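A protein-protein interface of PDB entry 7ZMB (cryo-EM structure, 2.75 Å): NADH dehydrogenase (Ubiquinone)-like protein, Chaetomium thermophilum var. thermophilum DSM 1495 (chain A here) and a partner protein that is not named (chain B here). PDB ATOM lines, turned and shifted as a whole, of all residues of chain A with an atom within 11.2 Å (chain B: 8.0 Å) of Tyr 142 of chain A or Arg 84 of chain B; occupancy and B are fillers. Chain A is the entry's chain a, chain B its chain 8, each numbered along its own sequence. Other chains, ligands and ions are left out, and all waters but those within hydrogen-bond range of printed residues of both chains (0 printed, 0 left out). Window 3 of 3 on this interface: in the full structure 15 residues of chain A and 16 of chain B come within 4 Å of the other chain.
Of the 14 printed residues of chain A, 3 touch a printed residue of chain B.
Printed residues of chain A that touch a printed residue of chain B: Tyr 142, Asp 144 and Arg 145.
Among the printed residues, Asp or Glu carboxylates within 4 Å of a Lys or Arg side-chain nitrogen of the other chain: Asp 144 of chain A with Arg 84 of chain B (3.2 Å).
The side-chain hydroxyl of Tyr 142 of chain A sits close to the guanidinium group of Arg 84 of chain B, at 3.4 Å.
The side-chain carboxylate (OD2) of Asp 144 of chain A lies within salt-bridge range of the guanidinium group (NE) of Arg 84 of chain B, 3.2 Å away.
The side-chain carboxylate (OD2) of Asp 144 of chain A sits at hydrogen-bond distance from the backbone NH (N) of Ser 85 of chain B, 2.9 Å away.
The side-chain carboxylate of Asp 144 of chain A sits close to the side-chain amide oxygen of Asn 86 of chain B (2.9 Å).
Tyr 142 of chain A touches just these residues of chain B: Arg 84 (3.1 Å) and Asn 86 (3.9 Å).
Of the printed residues of chain A, Arg 84 of chain B touches Tyr 142 (3.1 Å) and Asp 144 (3.2 Å).
No residue of chain B comes within 4 Å of Pro 143 of chain A.
No residue of chain A comes within 4 Å of Gly 82 of chain B.
Printed residues of chain A within 4 Å of Ala 83 of chain B: Asp 144.
Printed residues of chain A within 4 Å of Ser 85 of chain B: Asp 144 and Arg 145.
Of chain A, only Tyr 142 (3.9 Å), Asp 144 (2.9 Å) and Arg 145 (3.7 Å) come within 4 Å of Asn 86 of chain B.
Of the printed residues of chain B, Asp 144 of chain A touches Ala 83, Arg 84, Ser 85 and Asn 86.
Of the printed residues of chain B, Arg 145 of chain A touches Ser 85 (3.3 Å) and Asn 86 (3.7 Å).
Val 146 of chain A touches none of the printed residues of chain B.
Tyr 136 of chain A touches none of the printed residues of chain B.
The nearest residue of chain B that does not touch Tyr 142 of chain A is Ser 85 of chain B (7.2 Å).
The nearest residue of chain A that does not touch Arg 84 of chain B is Pro 143 of chain A (4.1 Å).
NH2 of Arg 84 of chain B lies within hydrogen-bond range of OD1 of Asn 86 of chain B (3.5 Å).
OH of Tyr 142 of chain A touches O of Asn 86 of chain B (3.9 Å).
O of Ala 83 of chain B touches OD2 of Asp 144 of chain A (3.95 Å).
CG of Arg 145 of chain A touches OG of Ser 85 of chain B (3.3 Å).
CD of Arg 145 of chain A touches CB of Asn 86 of chain B, at 3.7 Å.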
ATOM      1  N   LEU A 134       4.931   1.519  -5.945  1.00  0.00           N
ATOM      2  CA  LEU A 134       3.835   2.324  -6.471  1.00  0.00           C
ATOM      3  C   LEU A 134       4.326   3.698  -6.909  1.00  0.00           C
ATOM      4  O   LEU A 134       3.869   4.234  -7.926  1.00  0.00           O
ATOM      5  CB  LEU A 134       2.728   2.451  -5.425  1.00  0.00           C
ATOM      6  CG  LEU A 134       1.368   2.959  -5.909  1.00  0.00           C
ATOM      7  CD1 LEU A 134       0.249   2.274  -5.143  1.00  0.00           C
ATOM      8  CD2 LEU A 134       1.256   4.469  -5.772  1.00  0.00           C
ATOM      9  N   CYS A 135       5.254   4.286  -6.151  1.00  0.00           N
ATOM     10  CA  CYS A 135       5.793   5.591  -6.519  1.00  0.00           C
ATOM     11  C   CYS A 135       6.524   5.529  -7.852  1.00  0.00           C
ATOM     12  O   CYS A 135       6.436   6.460  -8.661  1.00  0.00           O
ATOM     13  CB  CYS A 135       6.723   6.103  -5.419  1.00  0.00           C
ATOM     14  SG  CYS A 135       7.641   7.597  -5.859  1.00  0.00           S
ATOM     15  N   TYR A 136       7.256   4.441  -8.097  1.00  0.00           N
ATOM     16  CA  TYR A 136       7.967   4.295  -9.363  1.00  0.00           C
ATOM     17  C   TYR A 136       6.997   4.231 -10.537  1.00  0.00           C
ATOM     18  O   TYR A 136       7.301   4.720 -11.631  1.00  0.00           O
ATOM     19  CB  TYR A 136       8.848   3.048  -9.325  1.00  0.00           C
ATOM     20  CG  TYR A 136       9.447   2.674 -10.660  1.00  0.00           C
ATOM     21  CD1 TYR A 136      10.218   3.581 -11.376  1.00  0.00           C
ATOM     22  CD2 TYR A 136       9.243   1.414 -11.205  1.00  0.00           C
ATOM     23  CE1 TYR A 136      10.767   3.242 -12.597  1.00  0.00           C
ATOM     24  CE2 TYR A 136       9.788   1.066 -12.424  1.00  0.00           C
ATOM     25  CZ  TYR A 136      10.549   1.983 -13.117  1.00  0.00           C
ATOM     26  OH  TYR A 136      11.094   1.640 -14.332  1.00  0.00           O
ATOM     27  N   VAL A 137       5.825   3.626 -10.328  1.00  0.00           N
ATOM     28  CA  VAL A 137       4.833   3.529 -11.396  1.00  0.00           C
ATOM     29  C   VAL A 137       4.358   4.915 -11.813  1.00  0.00           C
ATOM     30  O   VAL A 137       4.229   5.209 -13.008  1.00  0.00           O
ATOM     31  CB  VAL A 137       3.657   2.640 -10.950  1.00  0.00           C
ATOM     32  CG1 VAL A 137       2.573   2.621 -12.013  1.00  0.00           C
ATOM     33  CG2 VAL A 137       4.143   1.231 -10.657  1.00  0.00           C
ATOM     34  N   VAL A 138       4.095   5.786 -10.839  1.00  0.00           N
ATOM     35  CA  VAL A 138       3.576   7.114 -11.150  1.00  0.00           C
ATOM     36  C   VAL A 138       4.622   7.948 -11.877  1.00  0.00           C
ATOM     37  O   VAL A 138       4.293   8.737 -12.771  1.00  0.00           O
ATOM     38  CB  VAL A 138       3.090   7.808  -9.865  1.00  0.00           C
ATOM     39  CG1 VAL A 138       2.342   9.086 -10.205  1.00  0.00           C
ATOM     40  CG2 VAL A 138       2.210   6.868  -9.059  1.00  0.00           C
ATOM     41  N   LYS A 139       5.897   7.794 -11.509  1.00  0.00           N
ATOM     42  CA  LYS A 139       6.945   8.613 -12.108  1.00  0.00           C
ATOM     43  C   LYS A 139       7.059   8.364 -13.607  1.00  0.00           C
ATOM     44  O   LYS A 139       7.232   9.306 -14.388  1.00  0.00           O
ATOM     45  CB  LYS A 139       8.283   8.346 -11.421  1.00  0.00           C
ATOM     46  CG  LYS A 139       9.420   9.214 -11.933  1.00  0.00           C
ATOM     47  CD  LYS A 139      10.741   8.849 -11.275  1.00  0.00           C
ATOM     48  CE  LYS A 139      11.821   9.861 -11.619  1.00  0.00           C
ATOM     49  NZ  LYS A 139      12.081   9.921 -13.084  1.00  0.00           N
ATOM     50  N   LEU A 140       6.967   7.101 -14.028  1.00  0.00           N
ATOM     51  CA  LEU A 140       7.084   6.802 -15.449  1.00  0.00           C
ATOM     52  C   LEU A 140       5.833   7.203 -16.218  1.00  0.00           C
ATOM     53  O   LEU A 140       5.924   7.564 -17.397  1.00  0.00           O
ATOM     54  CB  LEU A 140       7.375   5.316 -15.651  1.00  0.00           C
ATOM     55  CG  LEU A 140       8.820   4.866 -15.418  1.00  0.00           C
ATOM     56  CD1 LEU A 140       9.060   3.502 -16.043  1.00  0.00           C
ATOM     57  CD2 LEU A 140       9.806   5.891 -15.961  1.00  0.00           C
ATOM     58  N   THR A 141       4.666   7.154 -15.578  1.00  0.00           N
ATOM     59  CA  THR A 141       3.389   7.431 -16.236  1.00  0.00           C
ATOM     60  C   THR A 141       2.623   8.462 -15.410  1.00  0.00           C
ATOM     61  O   THR A 141       1.915   8.111 -14.463  1.00  0.00           O
ATOM     62  CB  THR A 141       2.579   6.151 -16.414  1.00  0.00           C
ATOM     63  OG1 THR A 141       2.506   5.454 -15.164  1.00  0.00           O
ATOM     64  CG2 THR A 141       3.226   5.250 -17.455  1.00  0.00           C
ATOM     65  N   TYR A 142       2.764   9.736 -15.778  1.00  0.00           N
ATOM     66  CA  TYR A 142       1.992  10.801 -15.163  1.00  0.00           C
ATOM     67  C   TYR A 142       1.848  11.926 -16.176  1.00  0.00           C
ATOM     68  O   TYR A 142       2.814  12.238 -16.886  1.00  0.00           O
ATOM     69  CB  TYR A 142       2.631  11.324 -13.872  1.00  0.00           C
ATOM     70  CG  TYR A 142       3.890  12.142 -14.056  1.00  0.00           C
ATOM     71  CD1 TYR A 142       5.057  11.562 -14.528  1.00  0.00           C
ATOM     72  CD2 TYR A 142       3.914  13.493 -13.737  1.00  0.00           C
ATOM     73  CE1 TYR A 142       6.211  12.305 -14.688  1.00  0.00           C
ATOM     74  CE2 TYR A 142       5.061  14.244 -13.894  1.00  0.00           C
ATOM     75  CZ  TYR A 142       6.205  13.646 -14.370  1.00  0.00           C
ATOM     76  OH  TYR A 142       7.351  14.391 -14.528  1.00  0.00           O
ATOM     77  N   PRO A 143       0.670  12.537 -16.272  1.00  0.00           N
ATOM     78  CA  PRO A 143       0.435  13.523 -17.329  1.00  0.00           C
ATOM     79  C   PRO A 143       1.289  14.767 -17.154  1.00  0.00           C
ATOM     80  O   PRO A 143       1.613  15.180 -16.039  1.00  0.00           O
ATOM     81  CB  PRO A 143      -1.054  13.851 -17.180  1.00  0.00           C
ATOM     82  CG  PRO A 143      -1.348  13.566 -15.749  1.00  0.00           C
ATOM     83  CD  PRO A 143      -0.496  12.387 -15.387  1.00  0.00           C
ATOM     84  N   ASP A 144       1.651  15.364 -18.284  1.00  0.00           N
ATOM     85  CA  ASP A 144       2.369  16.626 -18.276  1.00  0.00           C
ATOM     86  C   ASP A 144       1.418  17.769 -17.938  1.00  0.00           C
ATOM     87  O   ASP A 144       0.193  17.627 -17.981  1.00  0.00           O
ATOM     88  CB  ASP A 144       3.037  16.876 -19.628  1.00  0.00           C
ATOM     89  CG  ASP A 144       4.211  17.829 -19.532  1.00  0.00           C
ATOM     90  OD1 ASP A 144       3.985  19.056 -19.579  1.00  0.00           O
ATOM     91  OD2 ASP A 144       5.358  17.351 -19.409  1.00  0.00           O
ATOM     92  N   ARG A 145       2.000  18.912 -17.592  1.00  0.00           N
ATOM     93  CA  ARG A 145       1.204  20.073 -17.225  1.00  0.00           C
ATOM     94  C   ARG A 145       0.393  20.571 -18.416  1.00  0.00           C
ATOM     95  O   ARG A 145       0.823  20.492 -19.570  1.00  0.00           O
ATOM     96  CB  ARG A 145       2.100  21.188 -16.686  1.00  0.00           C
ATOM     97  CG  ARG A 145       3.030  21.804 -17.715  1.00  0.00           C
ATOM     98  CD  ARG A 145       4.156  22.568 -17.039  1.00  0.00           C
ATOM     99  NE  ARG A 145       3.696  23.290 -15.855  1.00  0.00           N
ATOM    100  CZ  ARG A 145       2.977  24.409 -15.890  1.00  0.00           C
ATOM    101  NH1 ARG A 145       2.604  24.993 -14.761  1.00  0.00           N
ATOM    102  NH2 ARG A 145       2.629  24.941 -17.053  1.00  0.00           N
ATOM    103  N   VAL A 146      -0.801  21.079 -18.124  1.00  0.00           N
ATOM    104  CA  VAL A 146      -1.746  21.521 -19.140  1.00  0.00           C
ATOM    105  C   VAL A 146      -1.714  23.035 -19.311  1.00  0.00           C
ATOM    106  O   VAL A 146      -1.619  23.540 -20.430  1.00  0.00           O
ATOM    107  CB  VAL A 146      -3.175  21.035 -18.812  1.00  0.00           C
ATOM    108  CG1 VAL A 146      -4.166  21.590 -19.815  1.00  0.00           C
ATOM    109  CG2 VAL A 146      -3.225  19.519 -18.798  1.00  0.00           C
ATOM    110  N   ASP A 174      10.688  29.094 -19.465  1.00  0.00           N
ATOM    111  CA  ASP A 174       9.692  28.094 -19.100  1.00  0.00           C
ATOM    112  C   ASP A 174      10.160  26.684 -19.444  1.00  0.00           C
ATOM    113  O   ASP A 174       9.507  25.702 -19.089  1.00  0.00           O
ATOM    114  CB  ASP A 174       8.367  28.395 -19.800  1.00  0.00           C
ATOM    115  CG  ASP A 174       8.552  28.731 -21.264  1.00  0.00           C
ATOM    116  OD1 ASP A 174       9.713  28.795 -21.716  1.00  0.00           O
ATOM    117  OD2 ASP A 174       7.539  28.935 -21.965  1.00  0.00           O
ATOM    118  N   ARG B  77       4.854  22.836 -26.679  1.00  0.00           N
ATOM    119  CA  ARG B  77       5.327  21.467 -26.509  1.00  0.00           C
ATOM    120  C   ARG B  77       5.688  20.825 -27.839  1.00  0.00           C
ATOM    121  O   ARG B  77       6.444  19.847 -27.858  1.00  0.00           O
ATOM    122  CB  ARG B  77       4.280  20.617 -25.784  1.00  0.00           C
ATOM    123  CG  ARG B  77       3.006  20.352 -26.569  1.00  0.00           C
ATOM    124  CD  ARG B  77       1.985  19.615 -25.713  1.00  0.00           C
ATOM    125  NE  ARG B  77       0.783  19.257 -26.460  1.00  0.00           N
ATOM    126  CZ  ARG B  77      -0.271  20.052 -26.618  1.00  0.00           C
ATOM    127  NH1 ARG B  77      -1.319  19.633 -27.313  1.00  0.00           N
ATOM    128  NH2 ARG B  77      -0.278  21.264 -26.084  1.00  0.00           N
ATOM    129  N   LYS B  80       9.374  21.259 -28.456  1.00  0.00           N
ATOM    130  CA  LYS B  80      10.177  20.298 -27.714  1.00  0.00           C
ATOM    131  C   LYS B  80       9.943  18.864 -28.164  1.00  0.00           C
ATOM    132  O   LYS B  80      10.505  17.942 -27.563  1.00  0.00           O
ATOM    133  CB  LYS B  80       9.895  20.419 -26.214  1.00  0.00           C
ATOM    134  CG  LYS B  80      10.358  21.730 -25.599  1.00  0.00           C
ATOM    135  CD  LYS B  80      10.096  21.759 -24.103  1.00  0.00           C
ATOM    136  CE  LYS B  80      10.483  23.099 -23.503  1.00  0.00           C
ATOM    137  NZ  LYS B  80      11.955  23.321 -23.550  1.00  0.00           N
ATOM    138  N   GLY B  81       9.137  18.654 -29.199  1.00  0.00           N
ATOM    139  CA  GLY B  81       8.842  17.312 -29.665  1.00  0.00           C
ATOM    140  C   GLY B  81       8.069  16.474 -28.670  1.00  0.00           C
ATOM    141  O   GLY B  81       8.361  15.282 -28.511  1.00  0.00           O
ATOM    142  N   GLY B  82       7.086  17.068 -27.999  1.00  0.00           N
ATOM    143  CA  GLY B  82       6.313  16.342 -27.006  1.00  0.00           C
ATOM    144  C   GLY B  82       7.124  15.868 -25.822  1.00  0.00           C
ATOM    145  O   GLY B  82       6.850  14.792 -25.281  1.00  0.00           O
ATOM    146  N   ALA B  83       8.117  16.645 -25.403  1.00  0.00           N
ATOM    147  CA  ALA B  83       8.964  16.269 -24.280  1.00  0.00           C
ATOM    148  C   ALA B  83       8.261  16.625 -22.971  1.00  0.00           C
ATOM    149  O   ALA B  83       7.089  17.007 -22.948  1.00  0.00           O
ATOM    150  CB  ALA B  83      10.330  16.940 -24.399  1.00  0.00           C
ATOM    151  N   ARG B  84       8.980  16.502 -21.860  1.00  0.00           N
ATOM    152  CA  ARG B  84       8.428  16.794 -20.543  1.00  0.00           C
ATOM    153  C   ARG B  84       8.696  18.254 -20.201  1.00  0.00           C
ATOM    154  O   ARG B  84       9.854  18.659 -20.050  1.00  0.00           O
ATOM    155  CB  ARG B  84       9.033  15.870 -19.488  1.00  0.00           C
ATOM    156  CG  ARG B  84       8.999  14.398 -19.859  1.00  0.00           C
ATOM    157  CD  ARG B  84       7.594  13.940 -20.216  1.00  0.00           C
ATOM    158  NE  ARG B  84       6.597  14.420 -19.264  1.00  0.00           N
ATOM    159  CZ  ARG B  84       6.356  13.854 -18.088  1.00  0.00           C
ATOM    160  NH1 ARG B  84       7.041  12.782 -17.714  1.00  0.00           N
ATOM    161  NH2 ARG B  84       5.428  14.358 -17.286  1.00  0.00           N
ATOM    162  N   SER B  85       7.629  19.037 -20.078  1.00  0.00           N
ATOM    163  CA  SER B  85       7.741  20.458 -19.784  1.00  0.00           C
ATOM    164  C   SER B  85       7.733  20.760 -18.291  1.00  0.00           C
ATOM    165  O   SER B  85       7.880  21.926 -17.910  1.00  0.00           O
ATOM    166  CB  SER B  85       6.608  21.226 -20.470  1.00  0.00           C
ATOM    167  OG  SER B  85       5.350  20.870 -19.926  1.00  0.00           O
ATOM    168  N   ASN B  86       7.570  19.750 -17.444  1.00  0.00           N
ATOM    169  CA  ASN B  86       7.561  19.958 -16.001  1.00  0.00           C
ATOM    170  C   ASN B  86       8.474  18.962 -15.296  1.00  0.00           C
ATOM    171  O   ASN B  86       8.677  17.845 -15.773  1.00  0.00           O
ATOM    172  CB  ASN B  86       6.138  19.848 -15.451  1.00  0.00           C
ATOM    173  CG  ASN B  86       5.525  18.482 -15.691  1.00  0.00           C
ATOM    174  OD1 ASN B  86       5.962  17.737 -16.568  1.00  0.00           O
ATOM    175  ND2 ASN B  86       4.506  18.147 -14.910  1.00  0.00           N
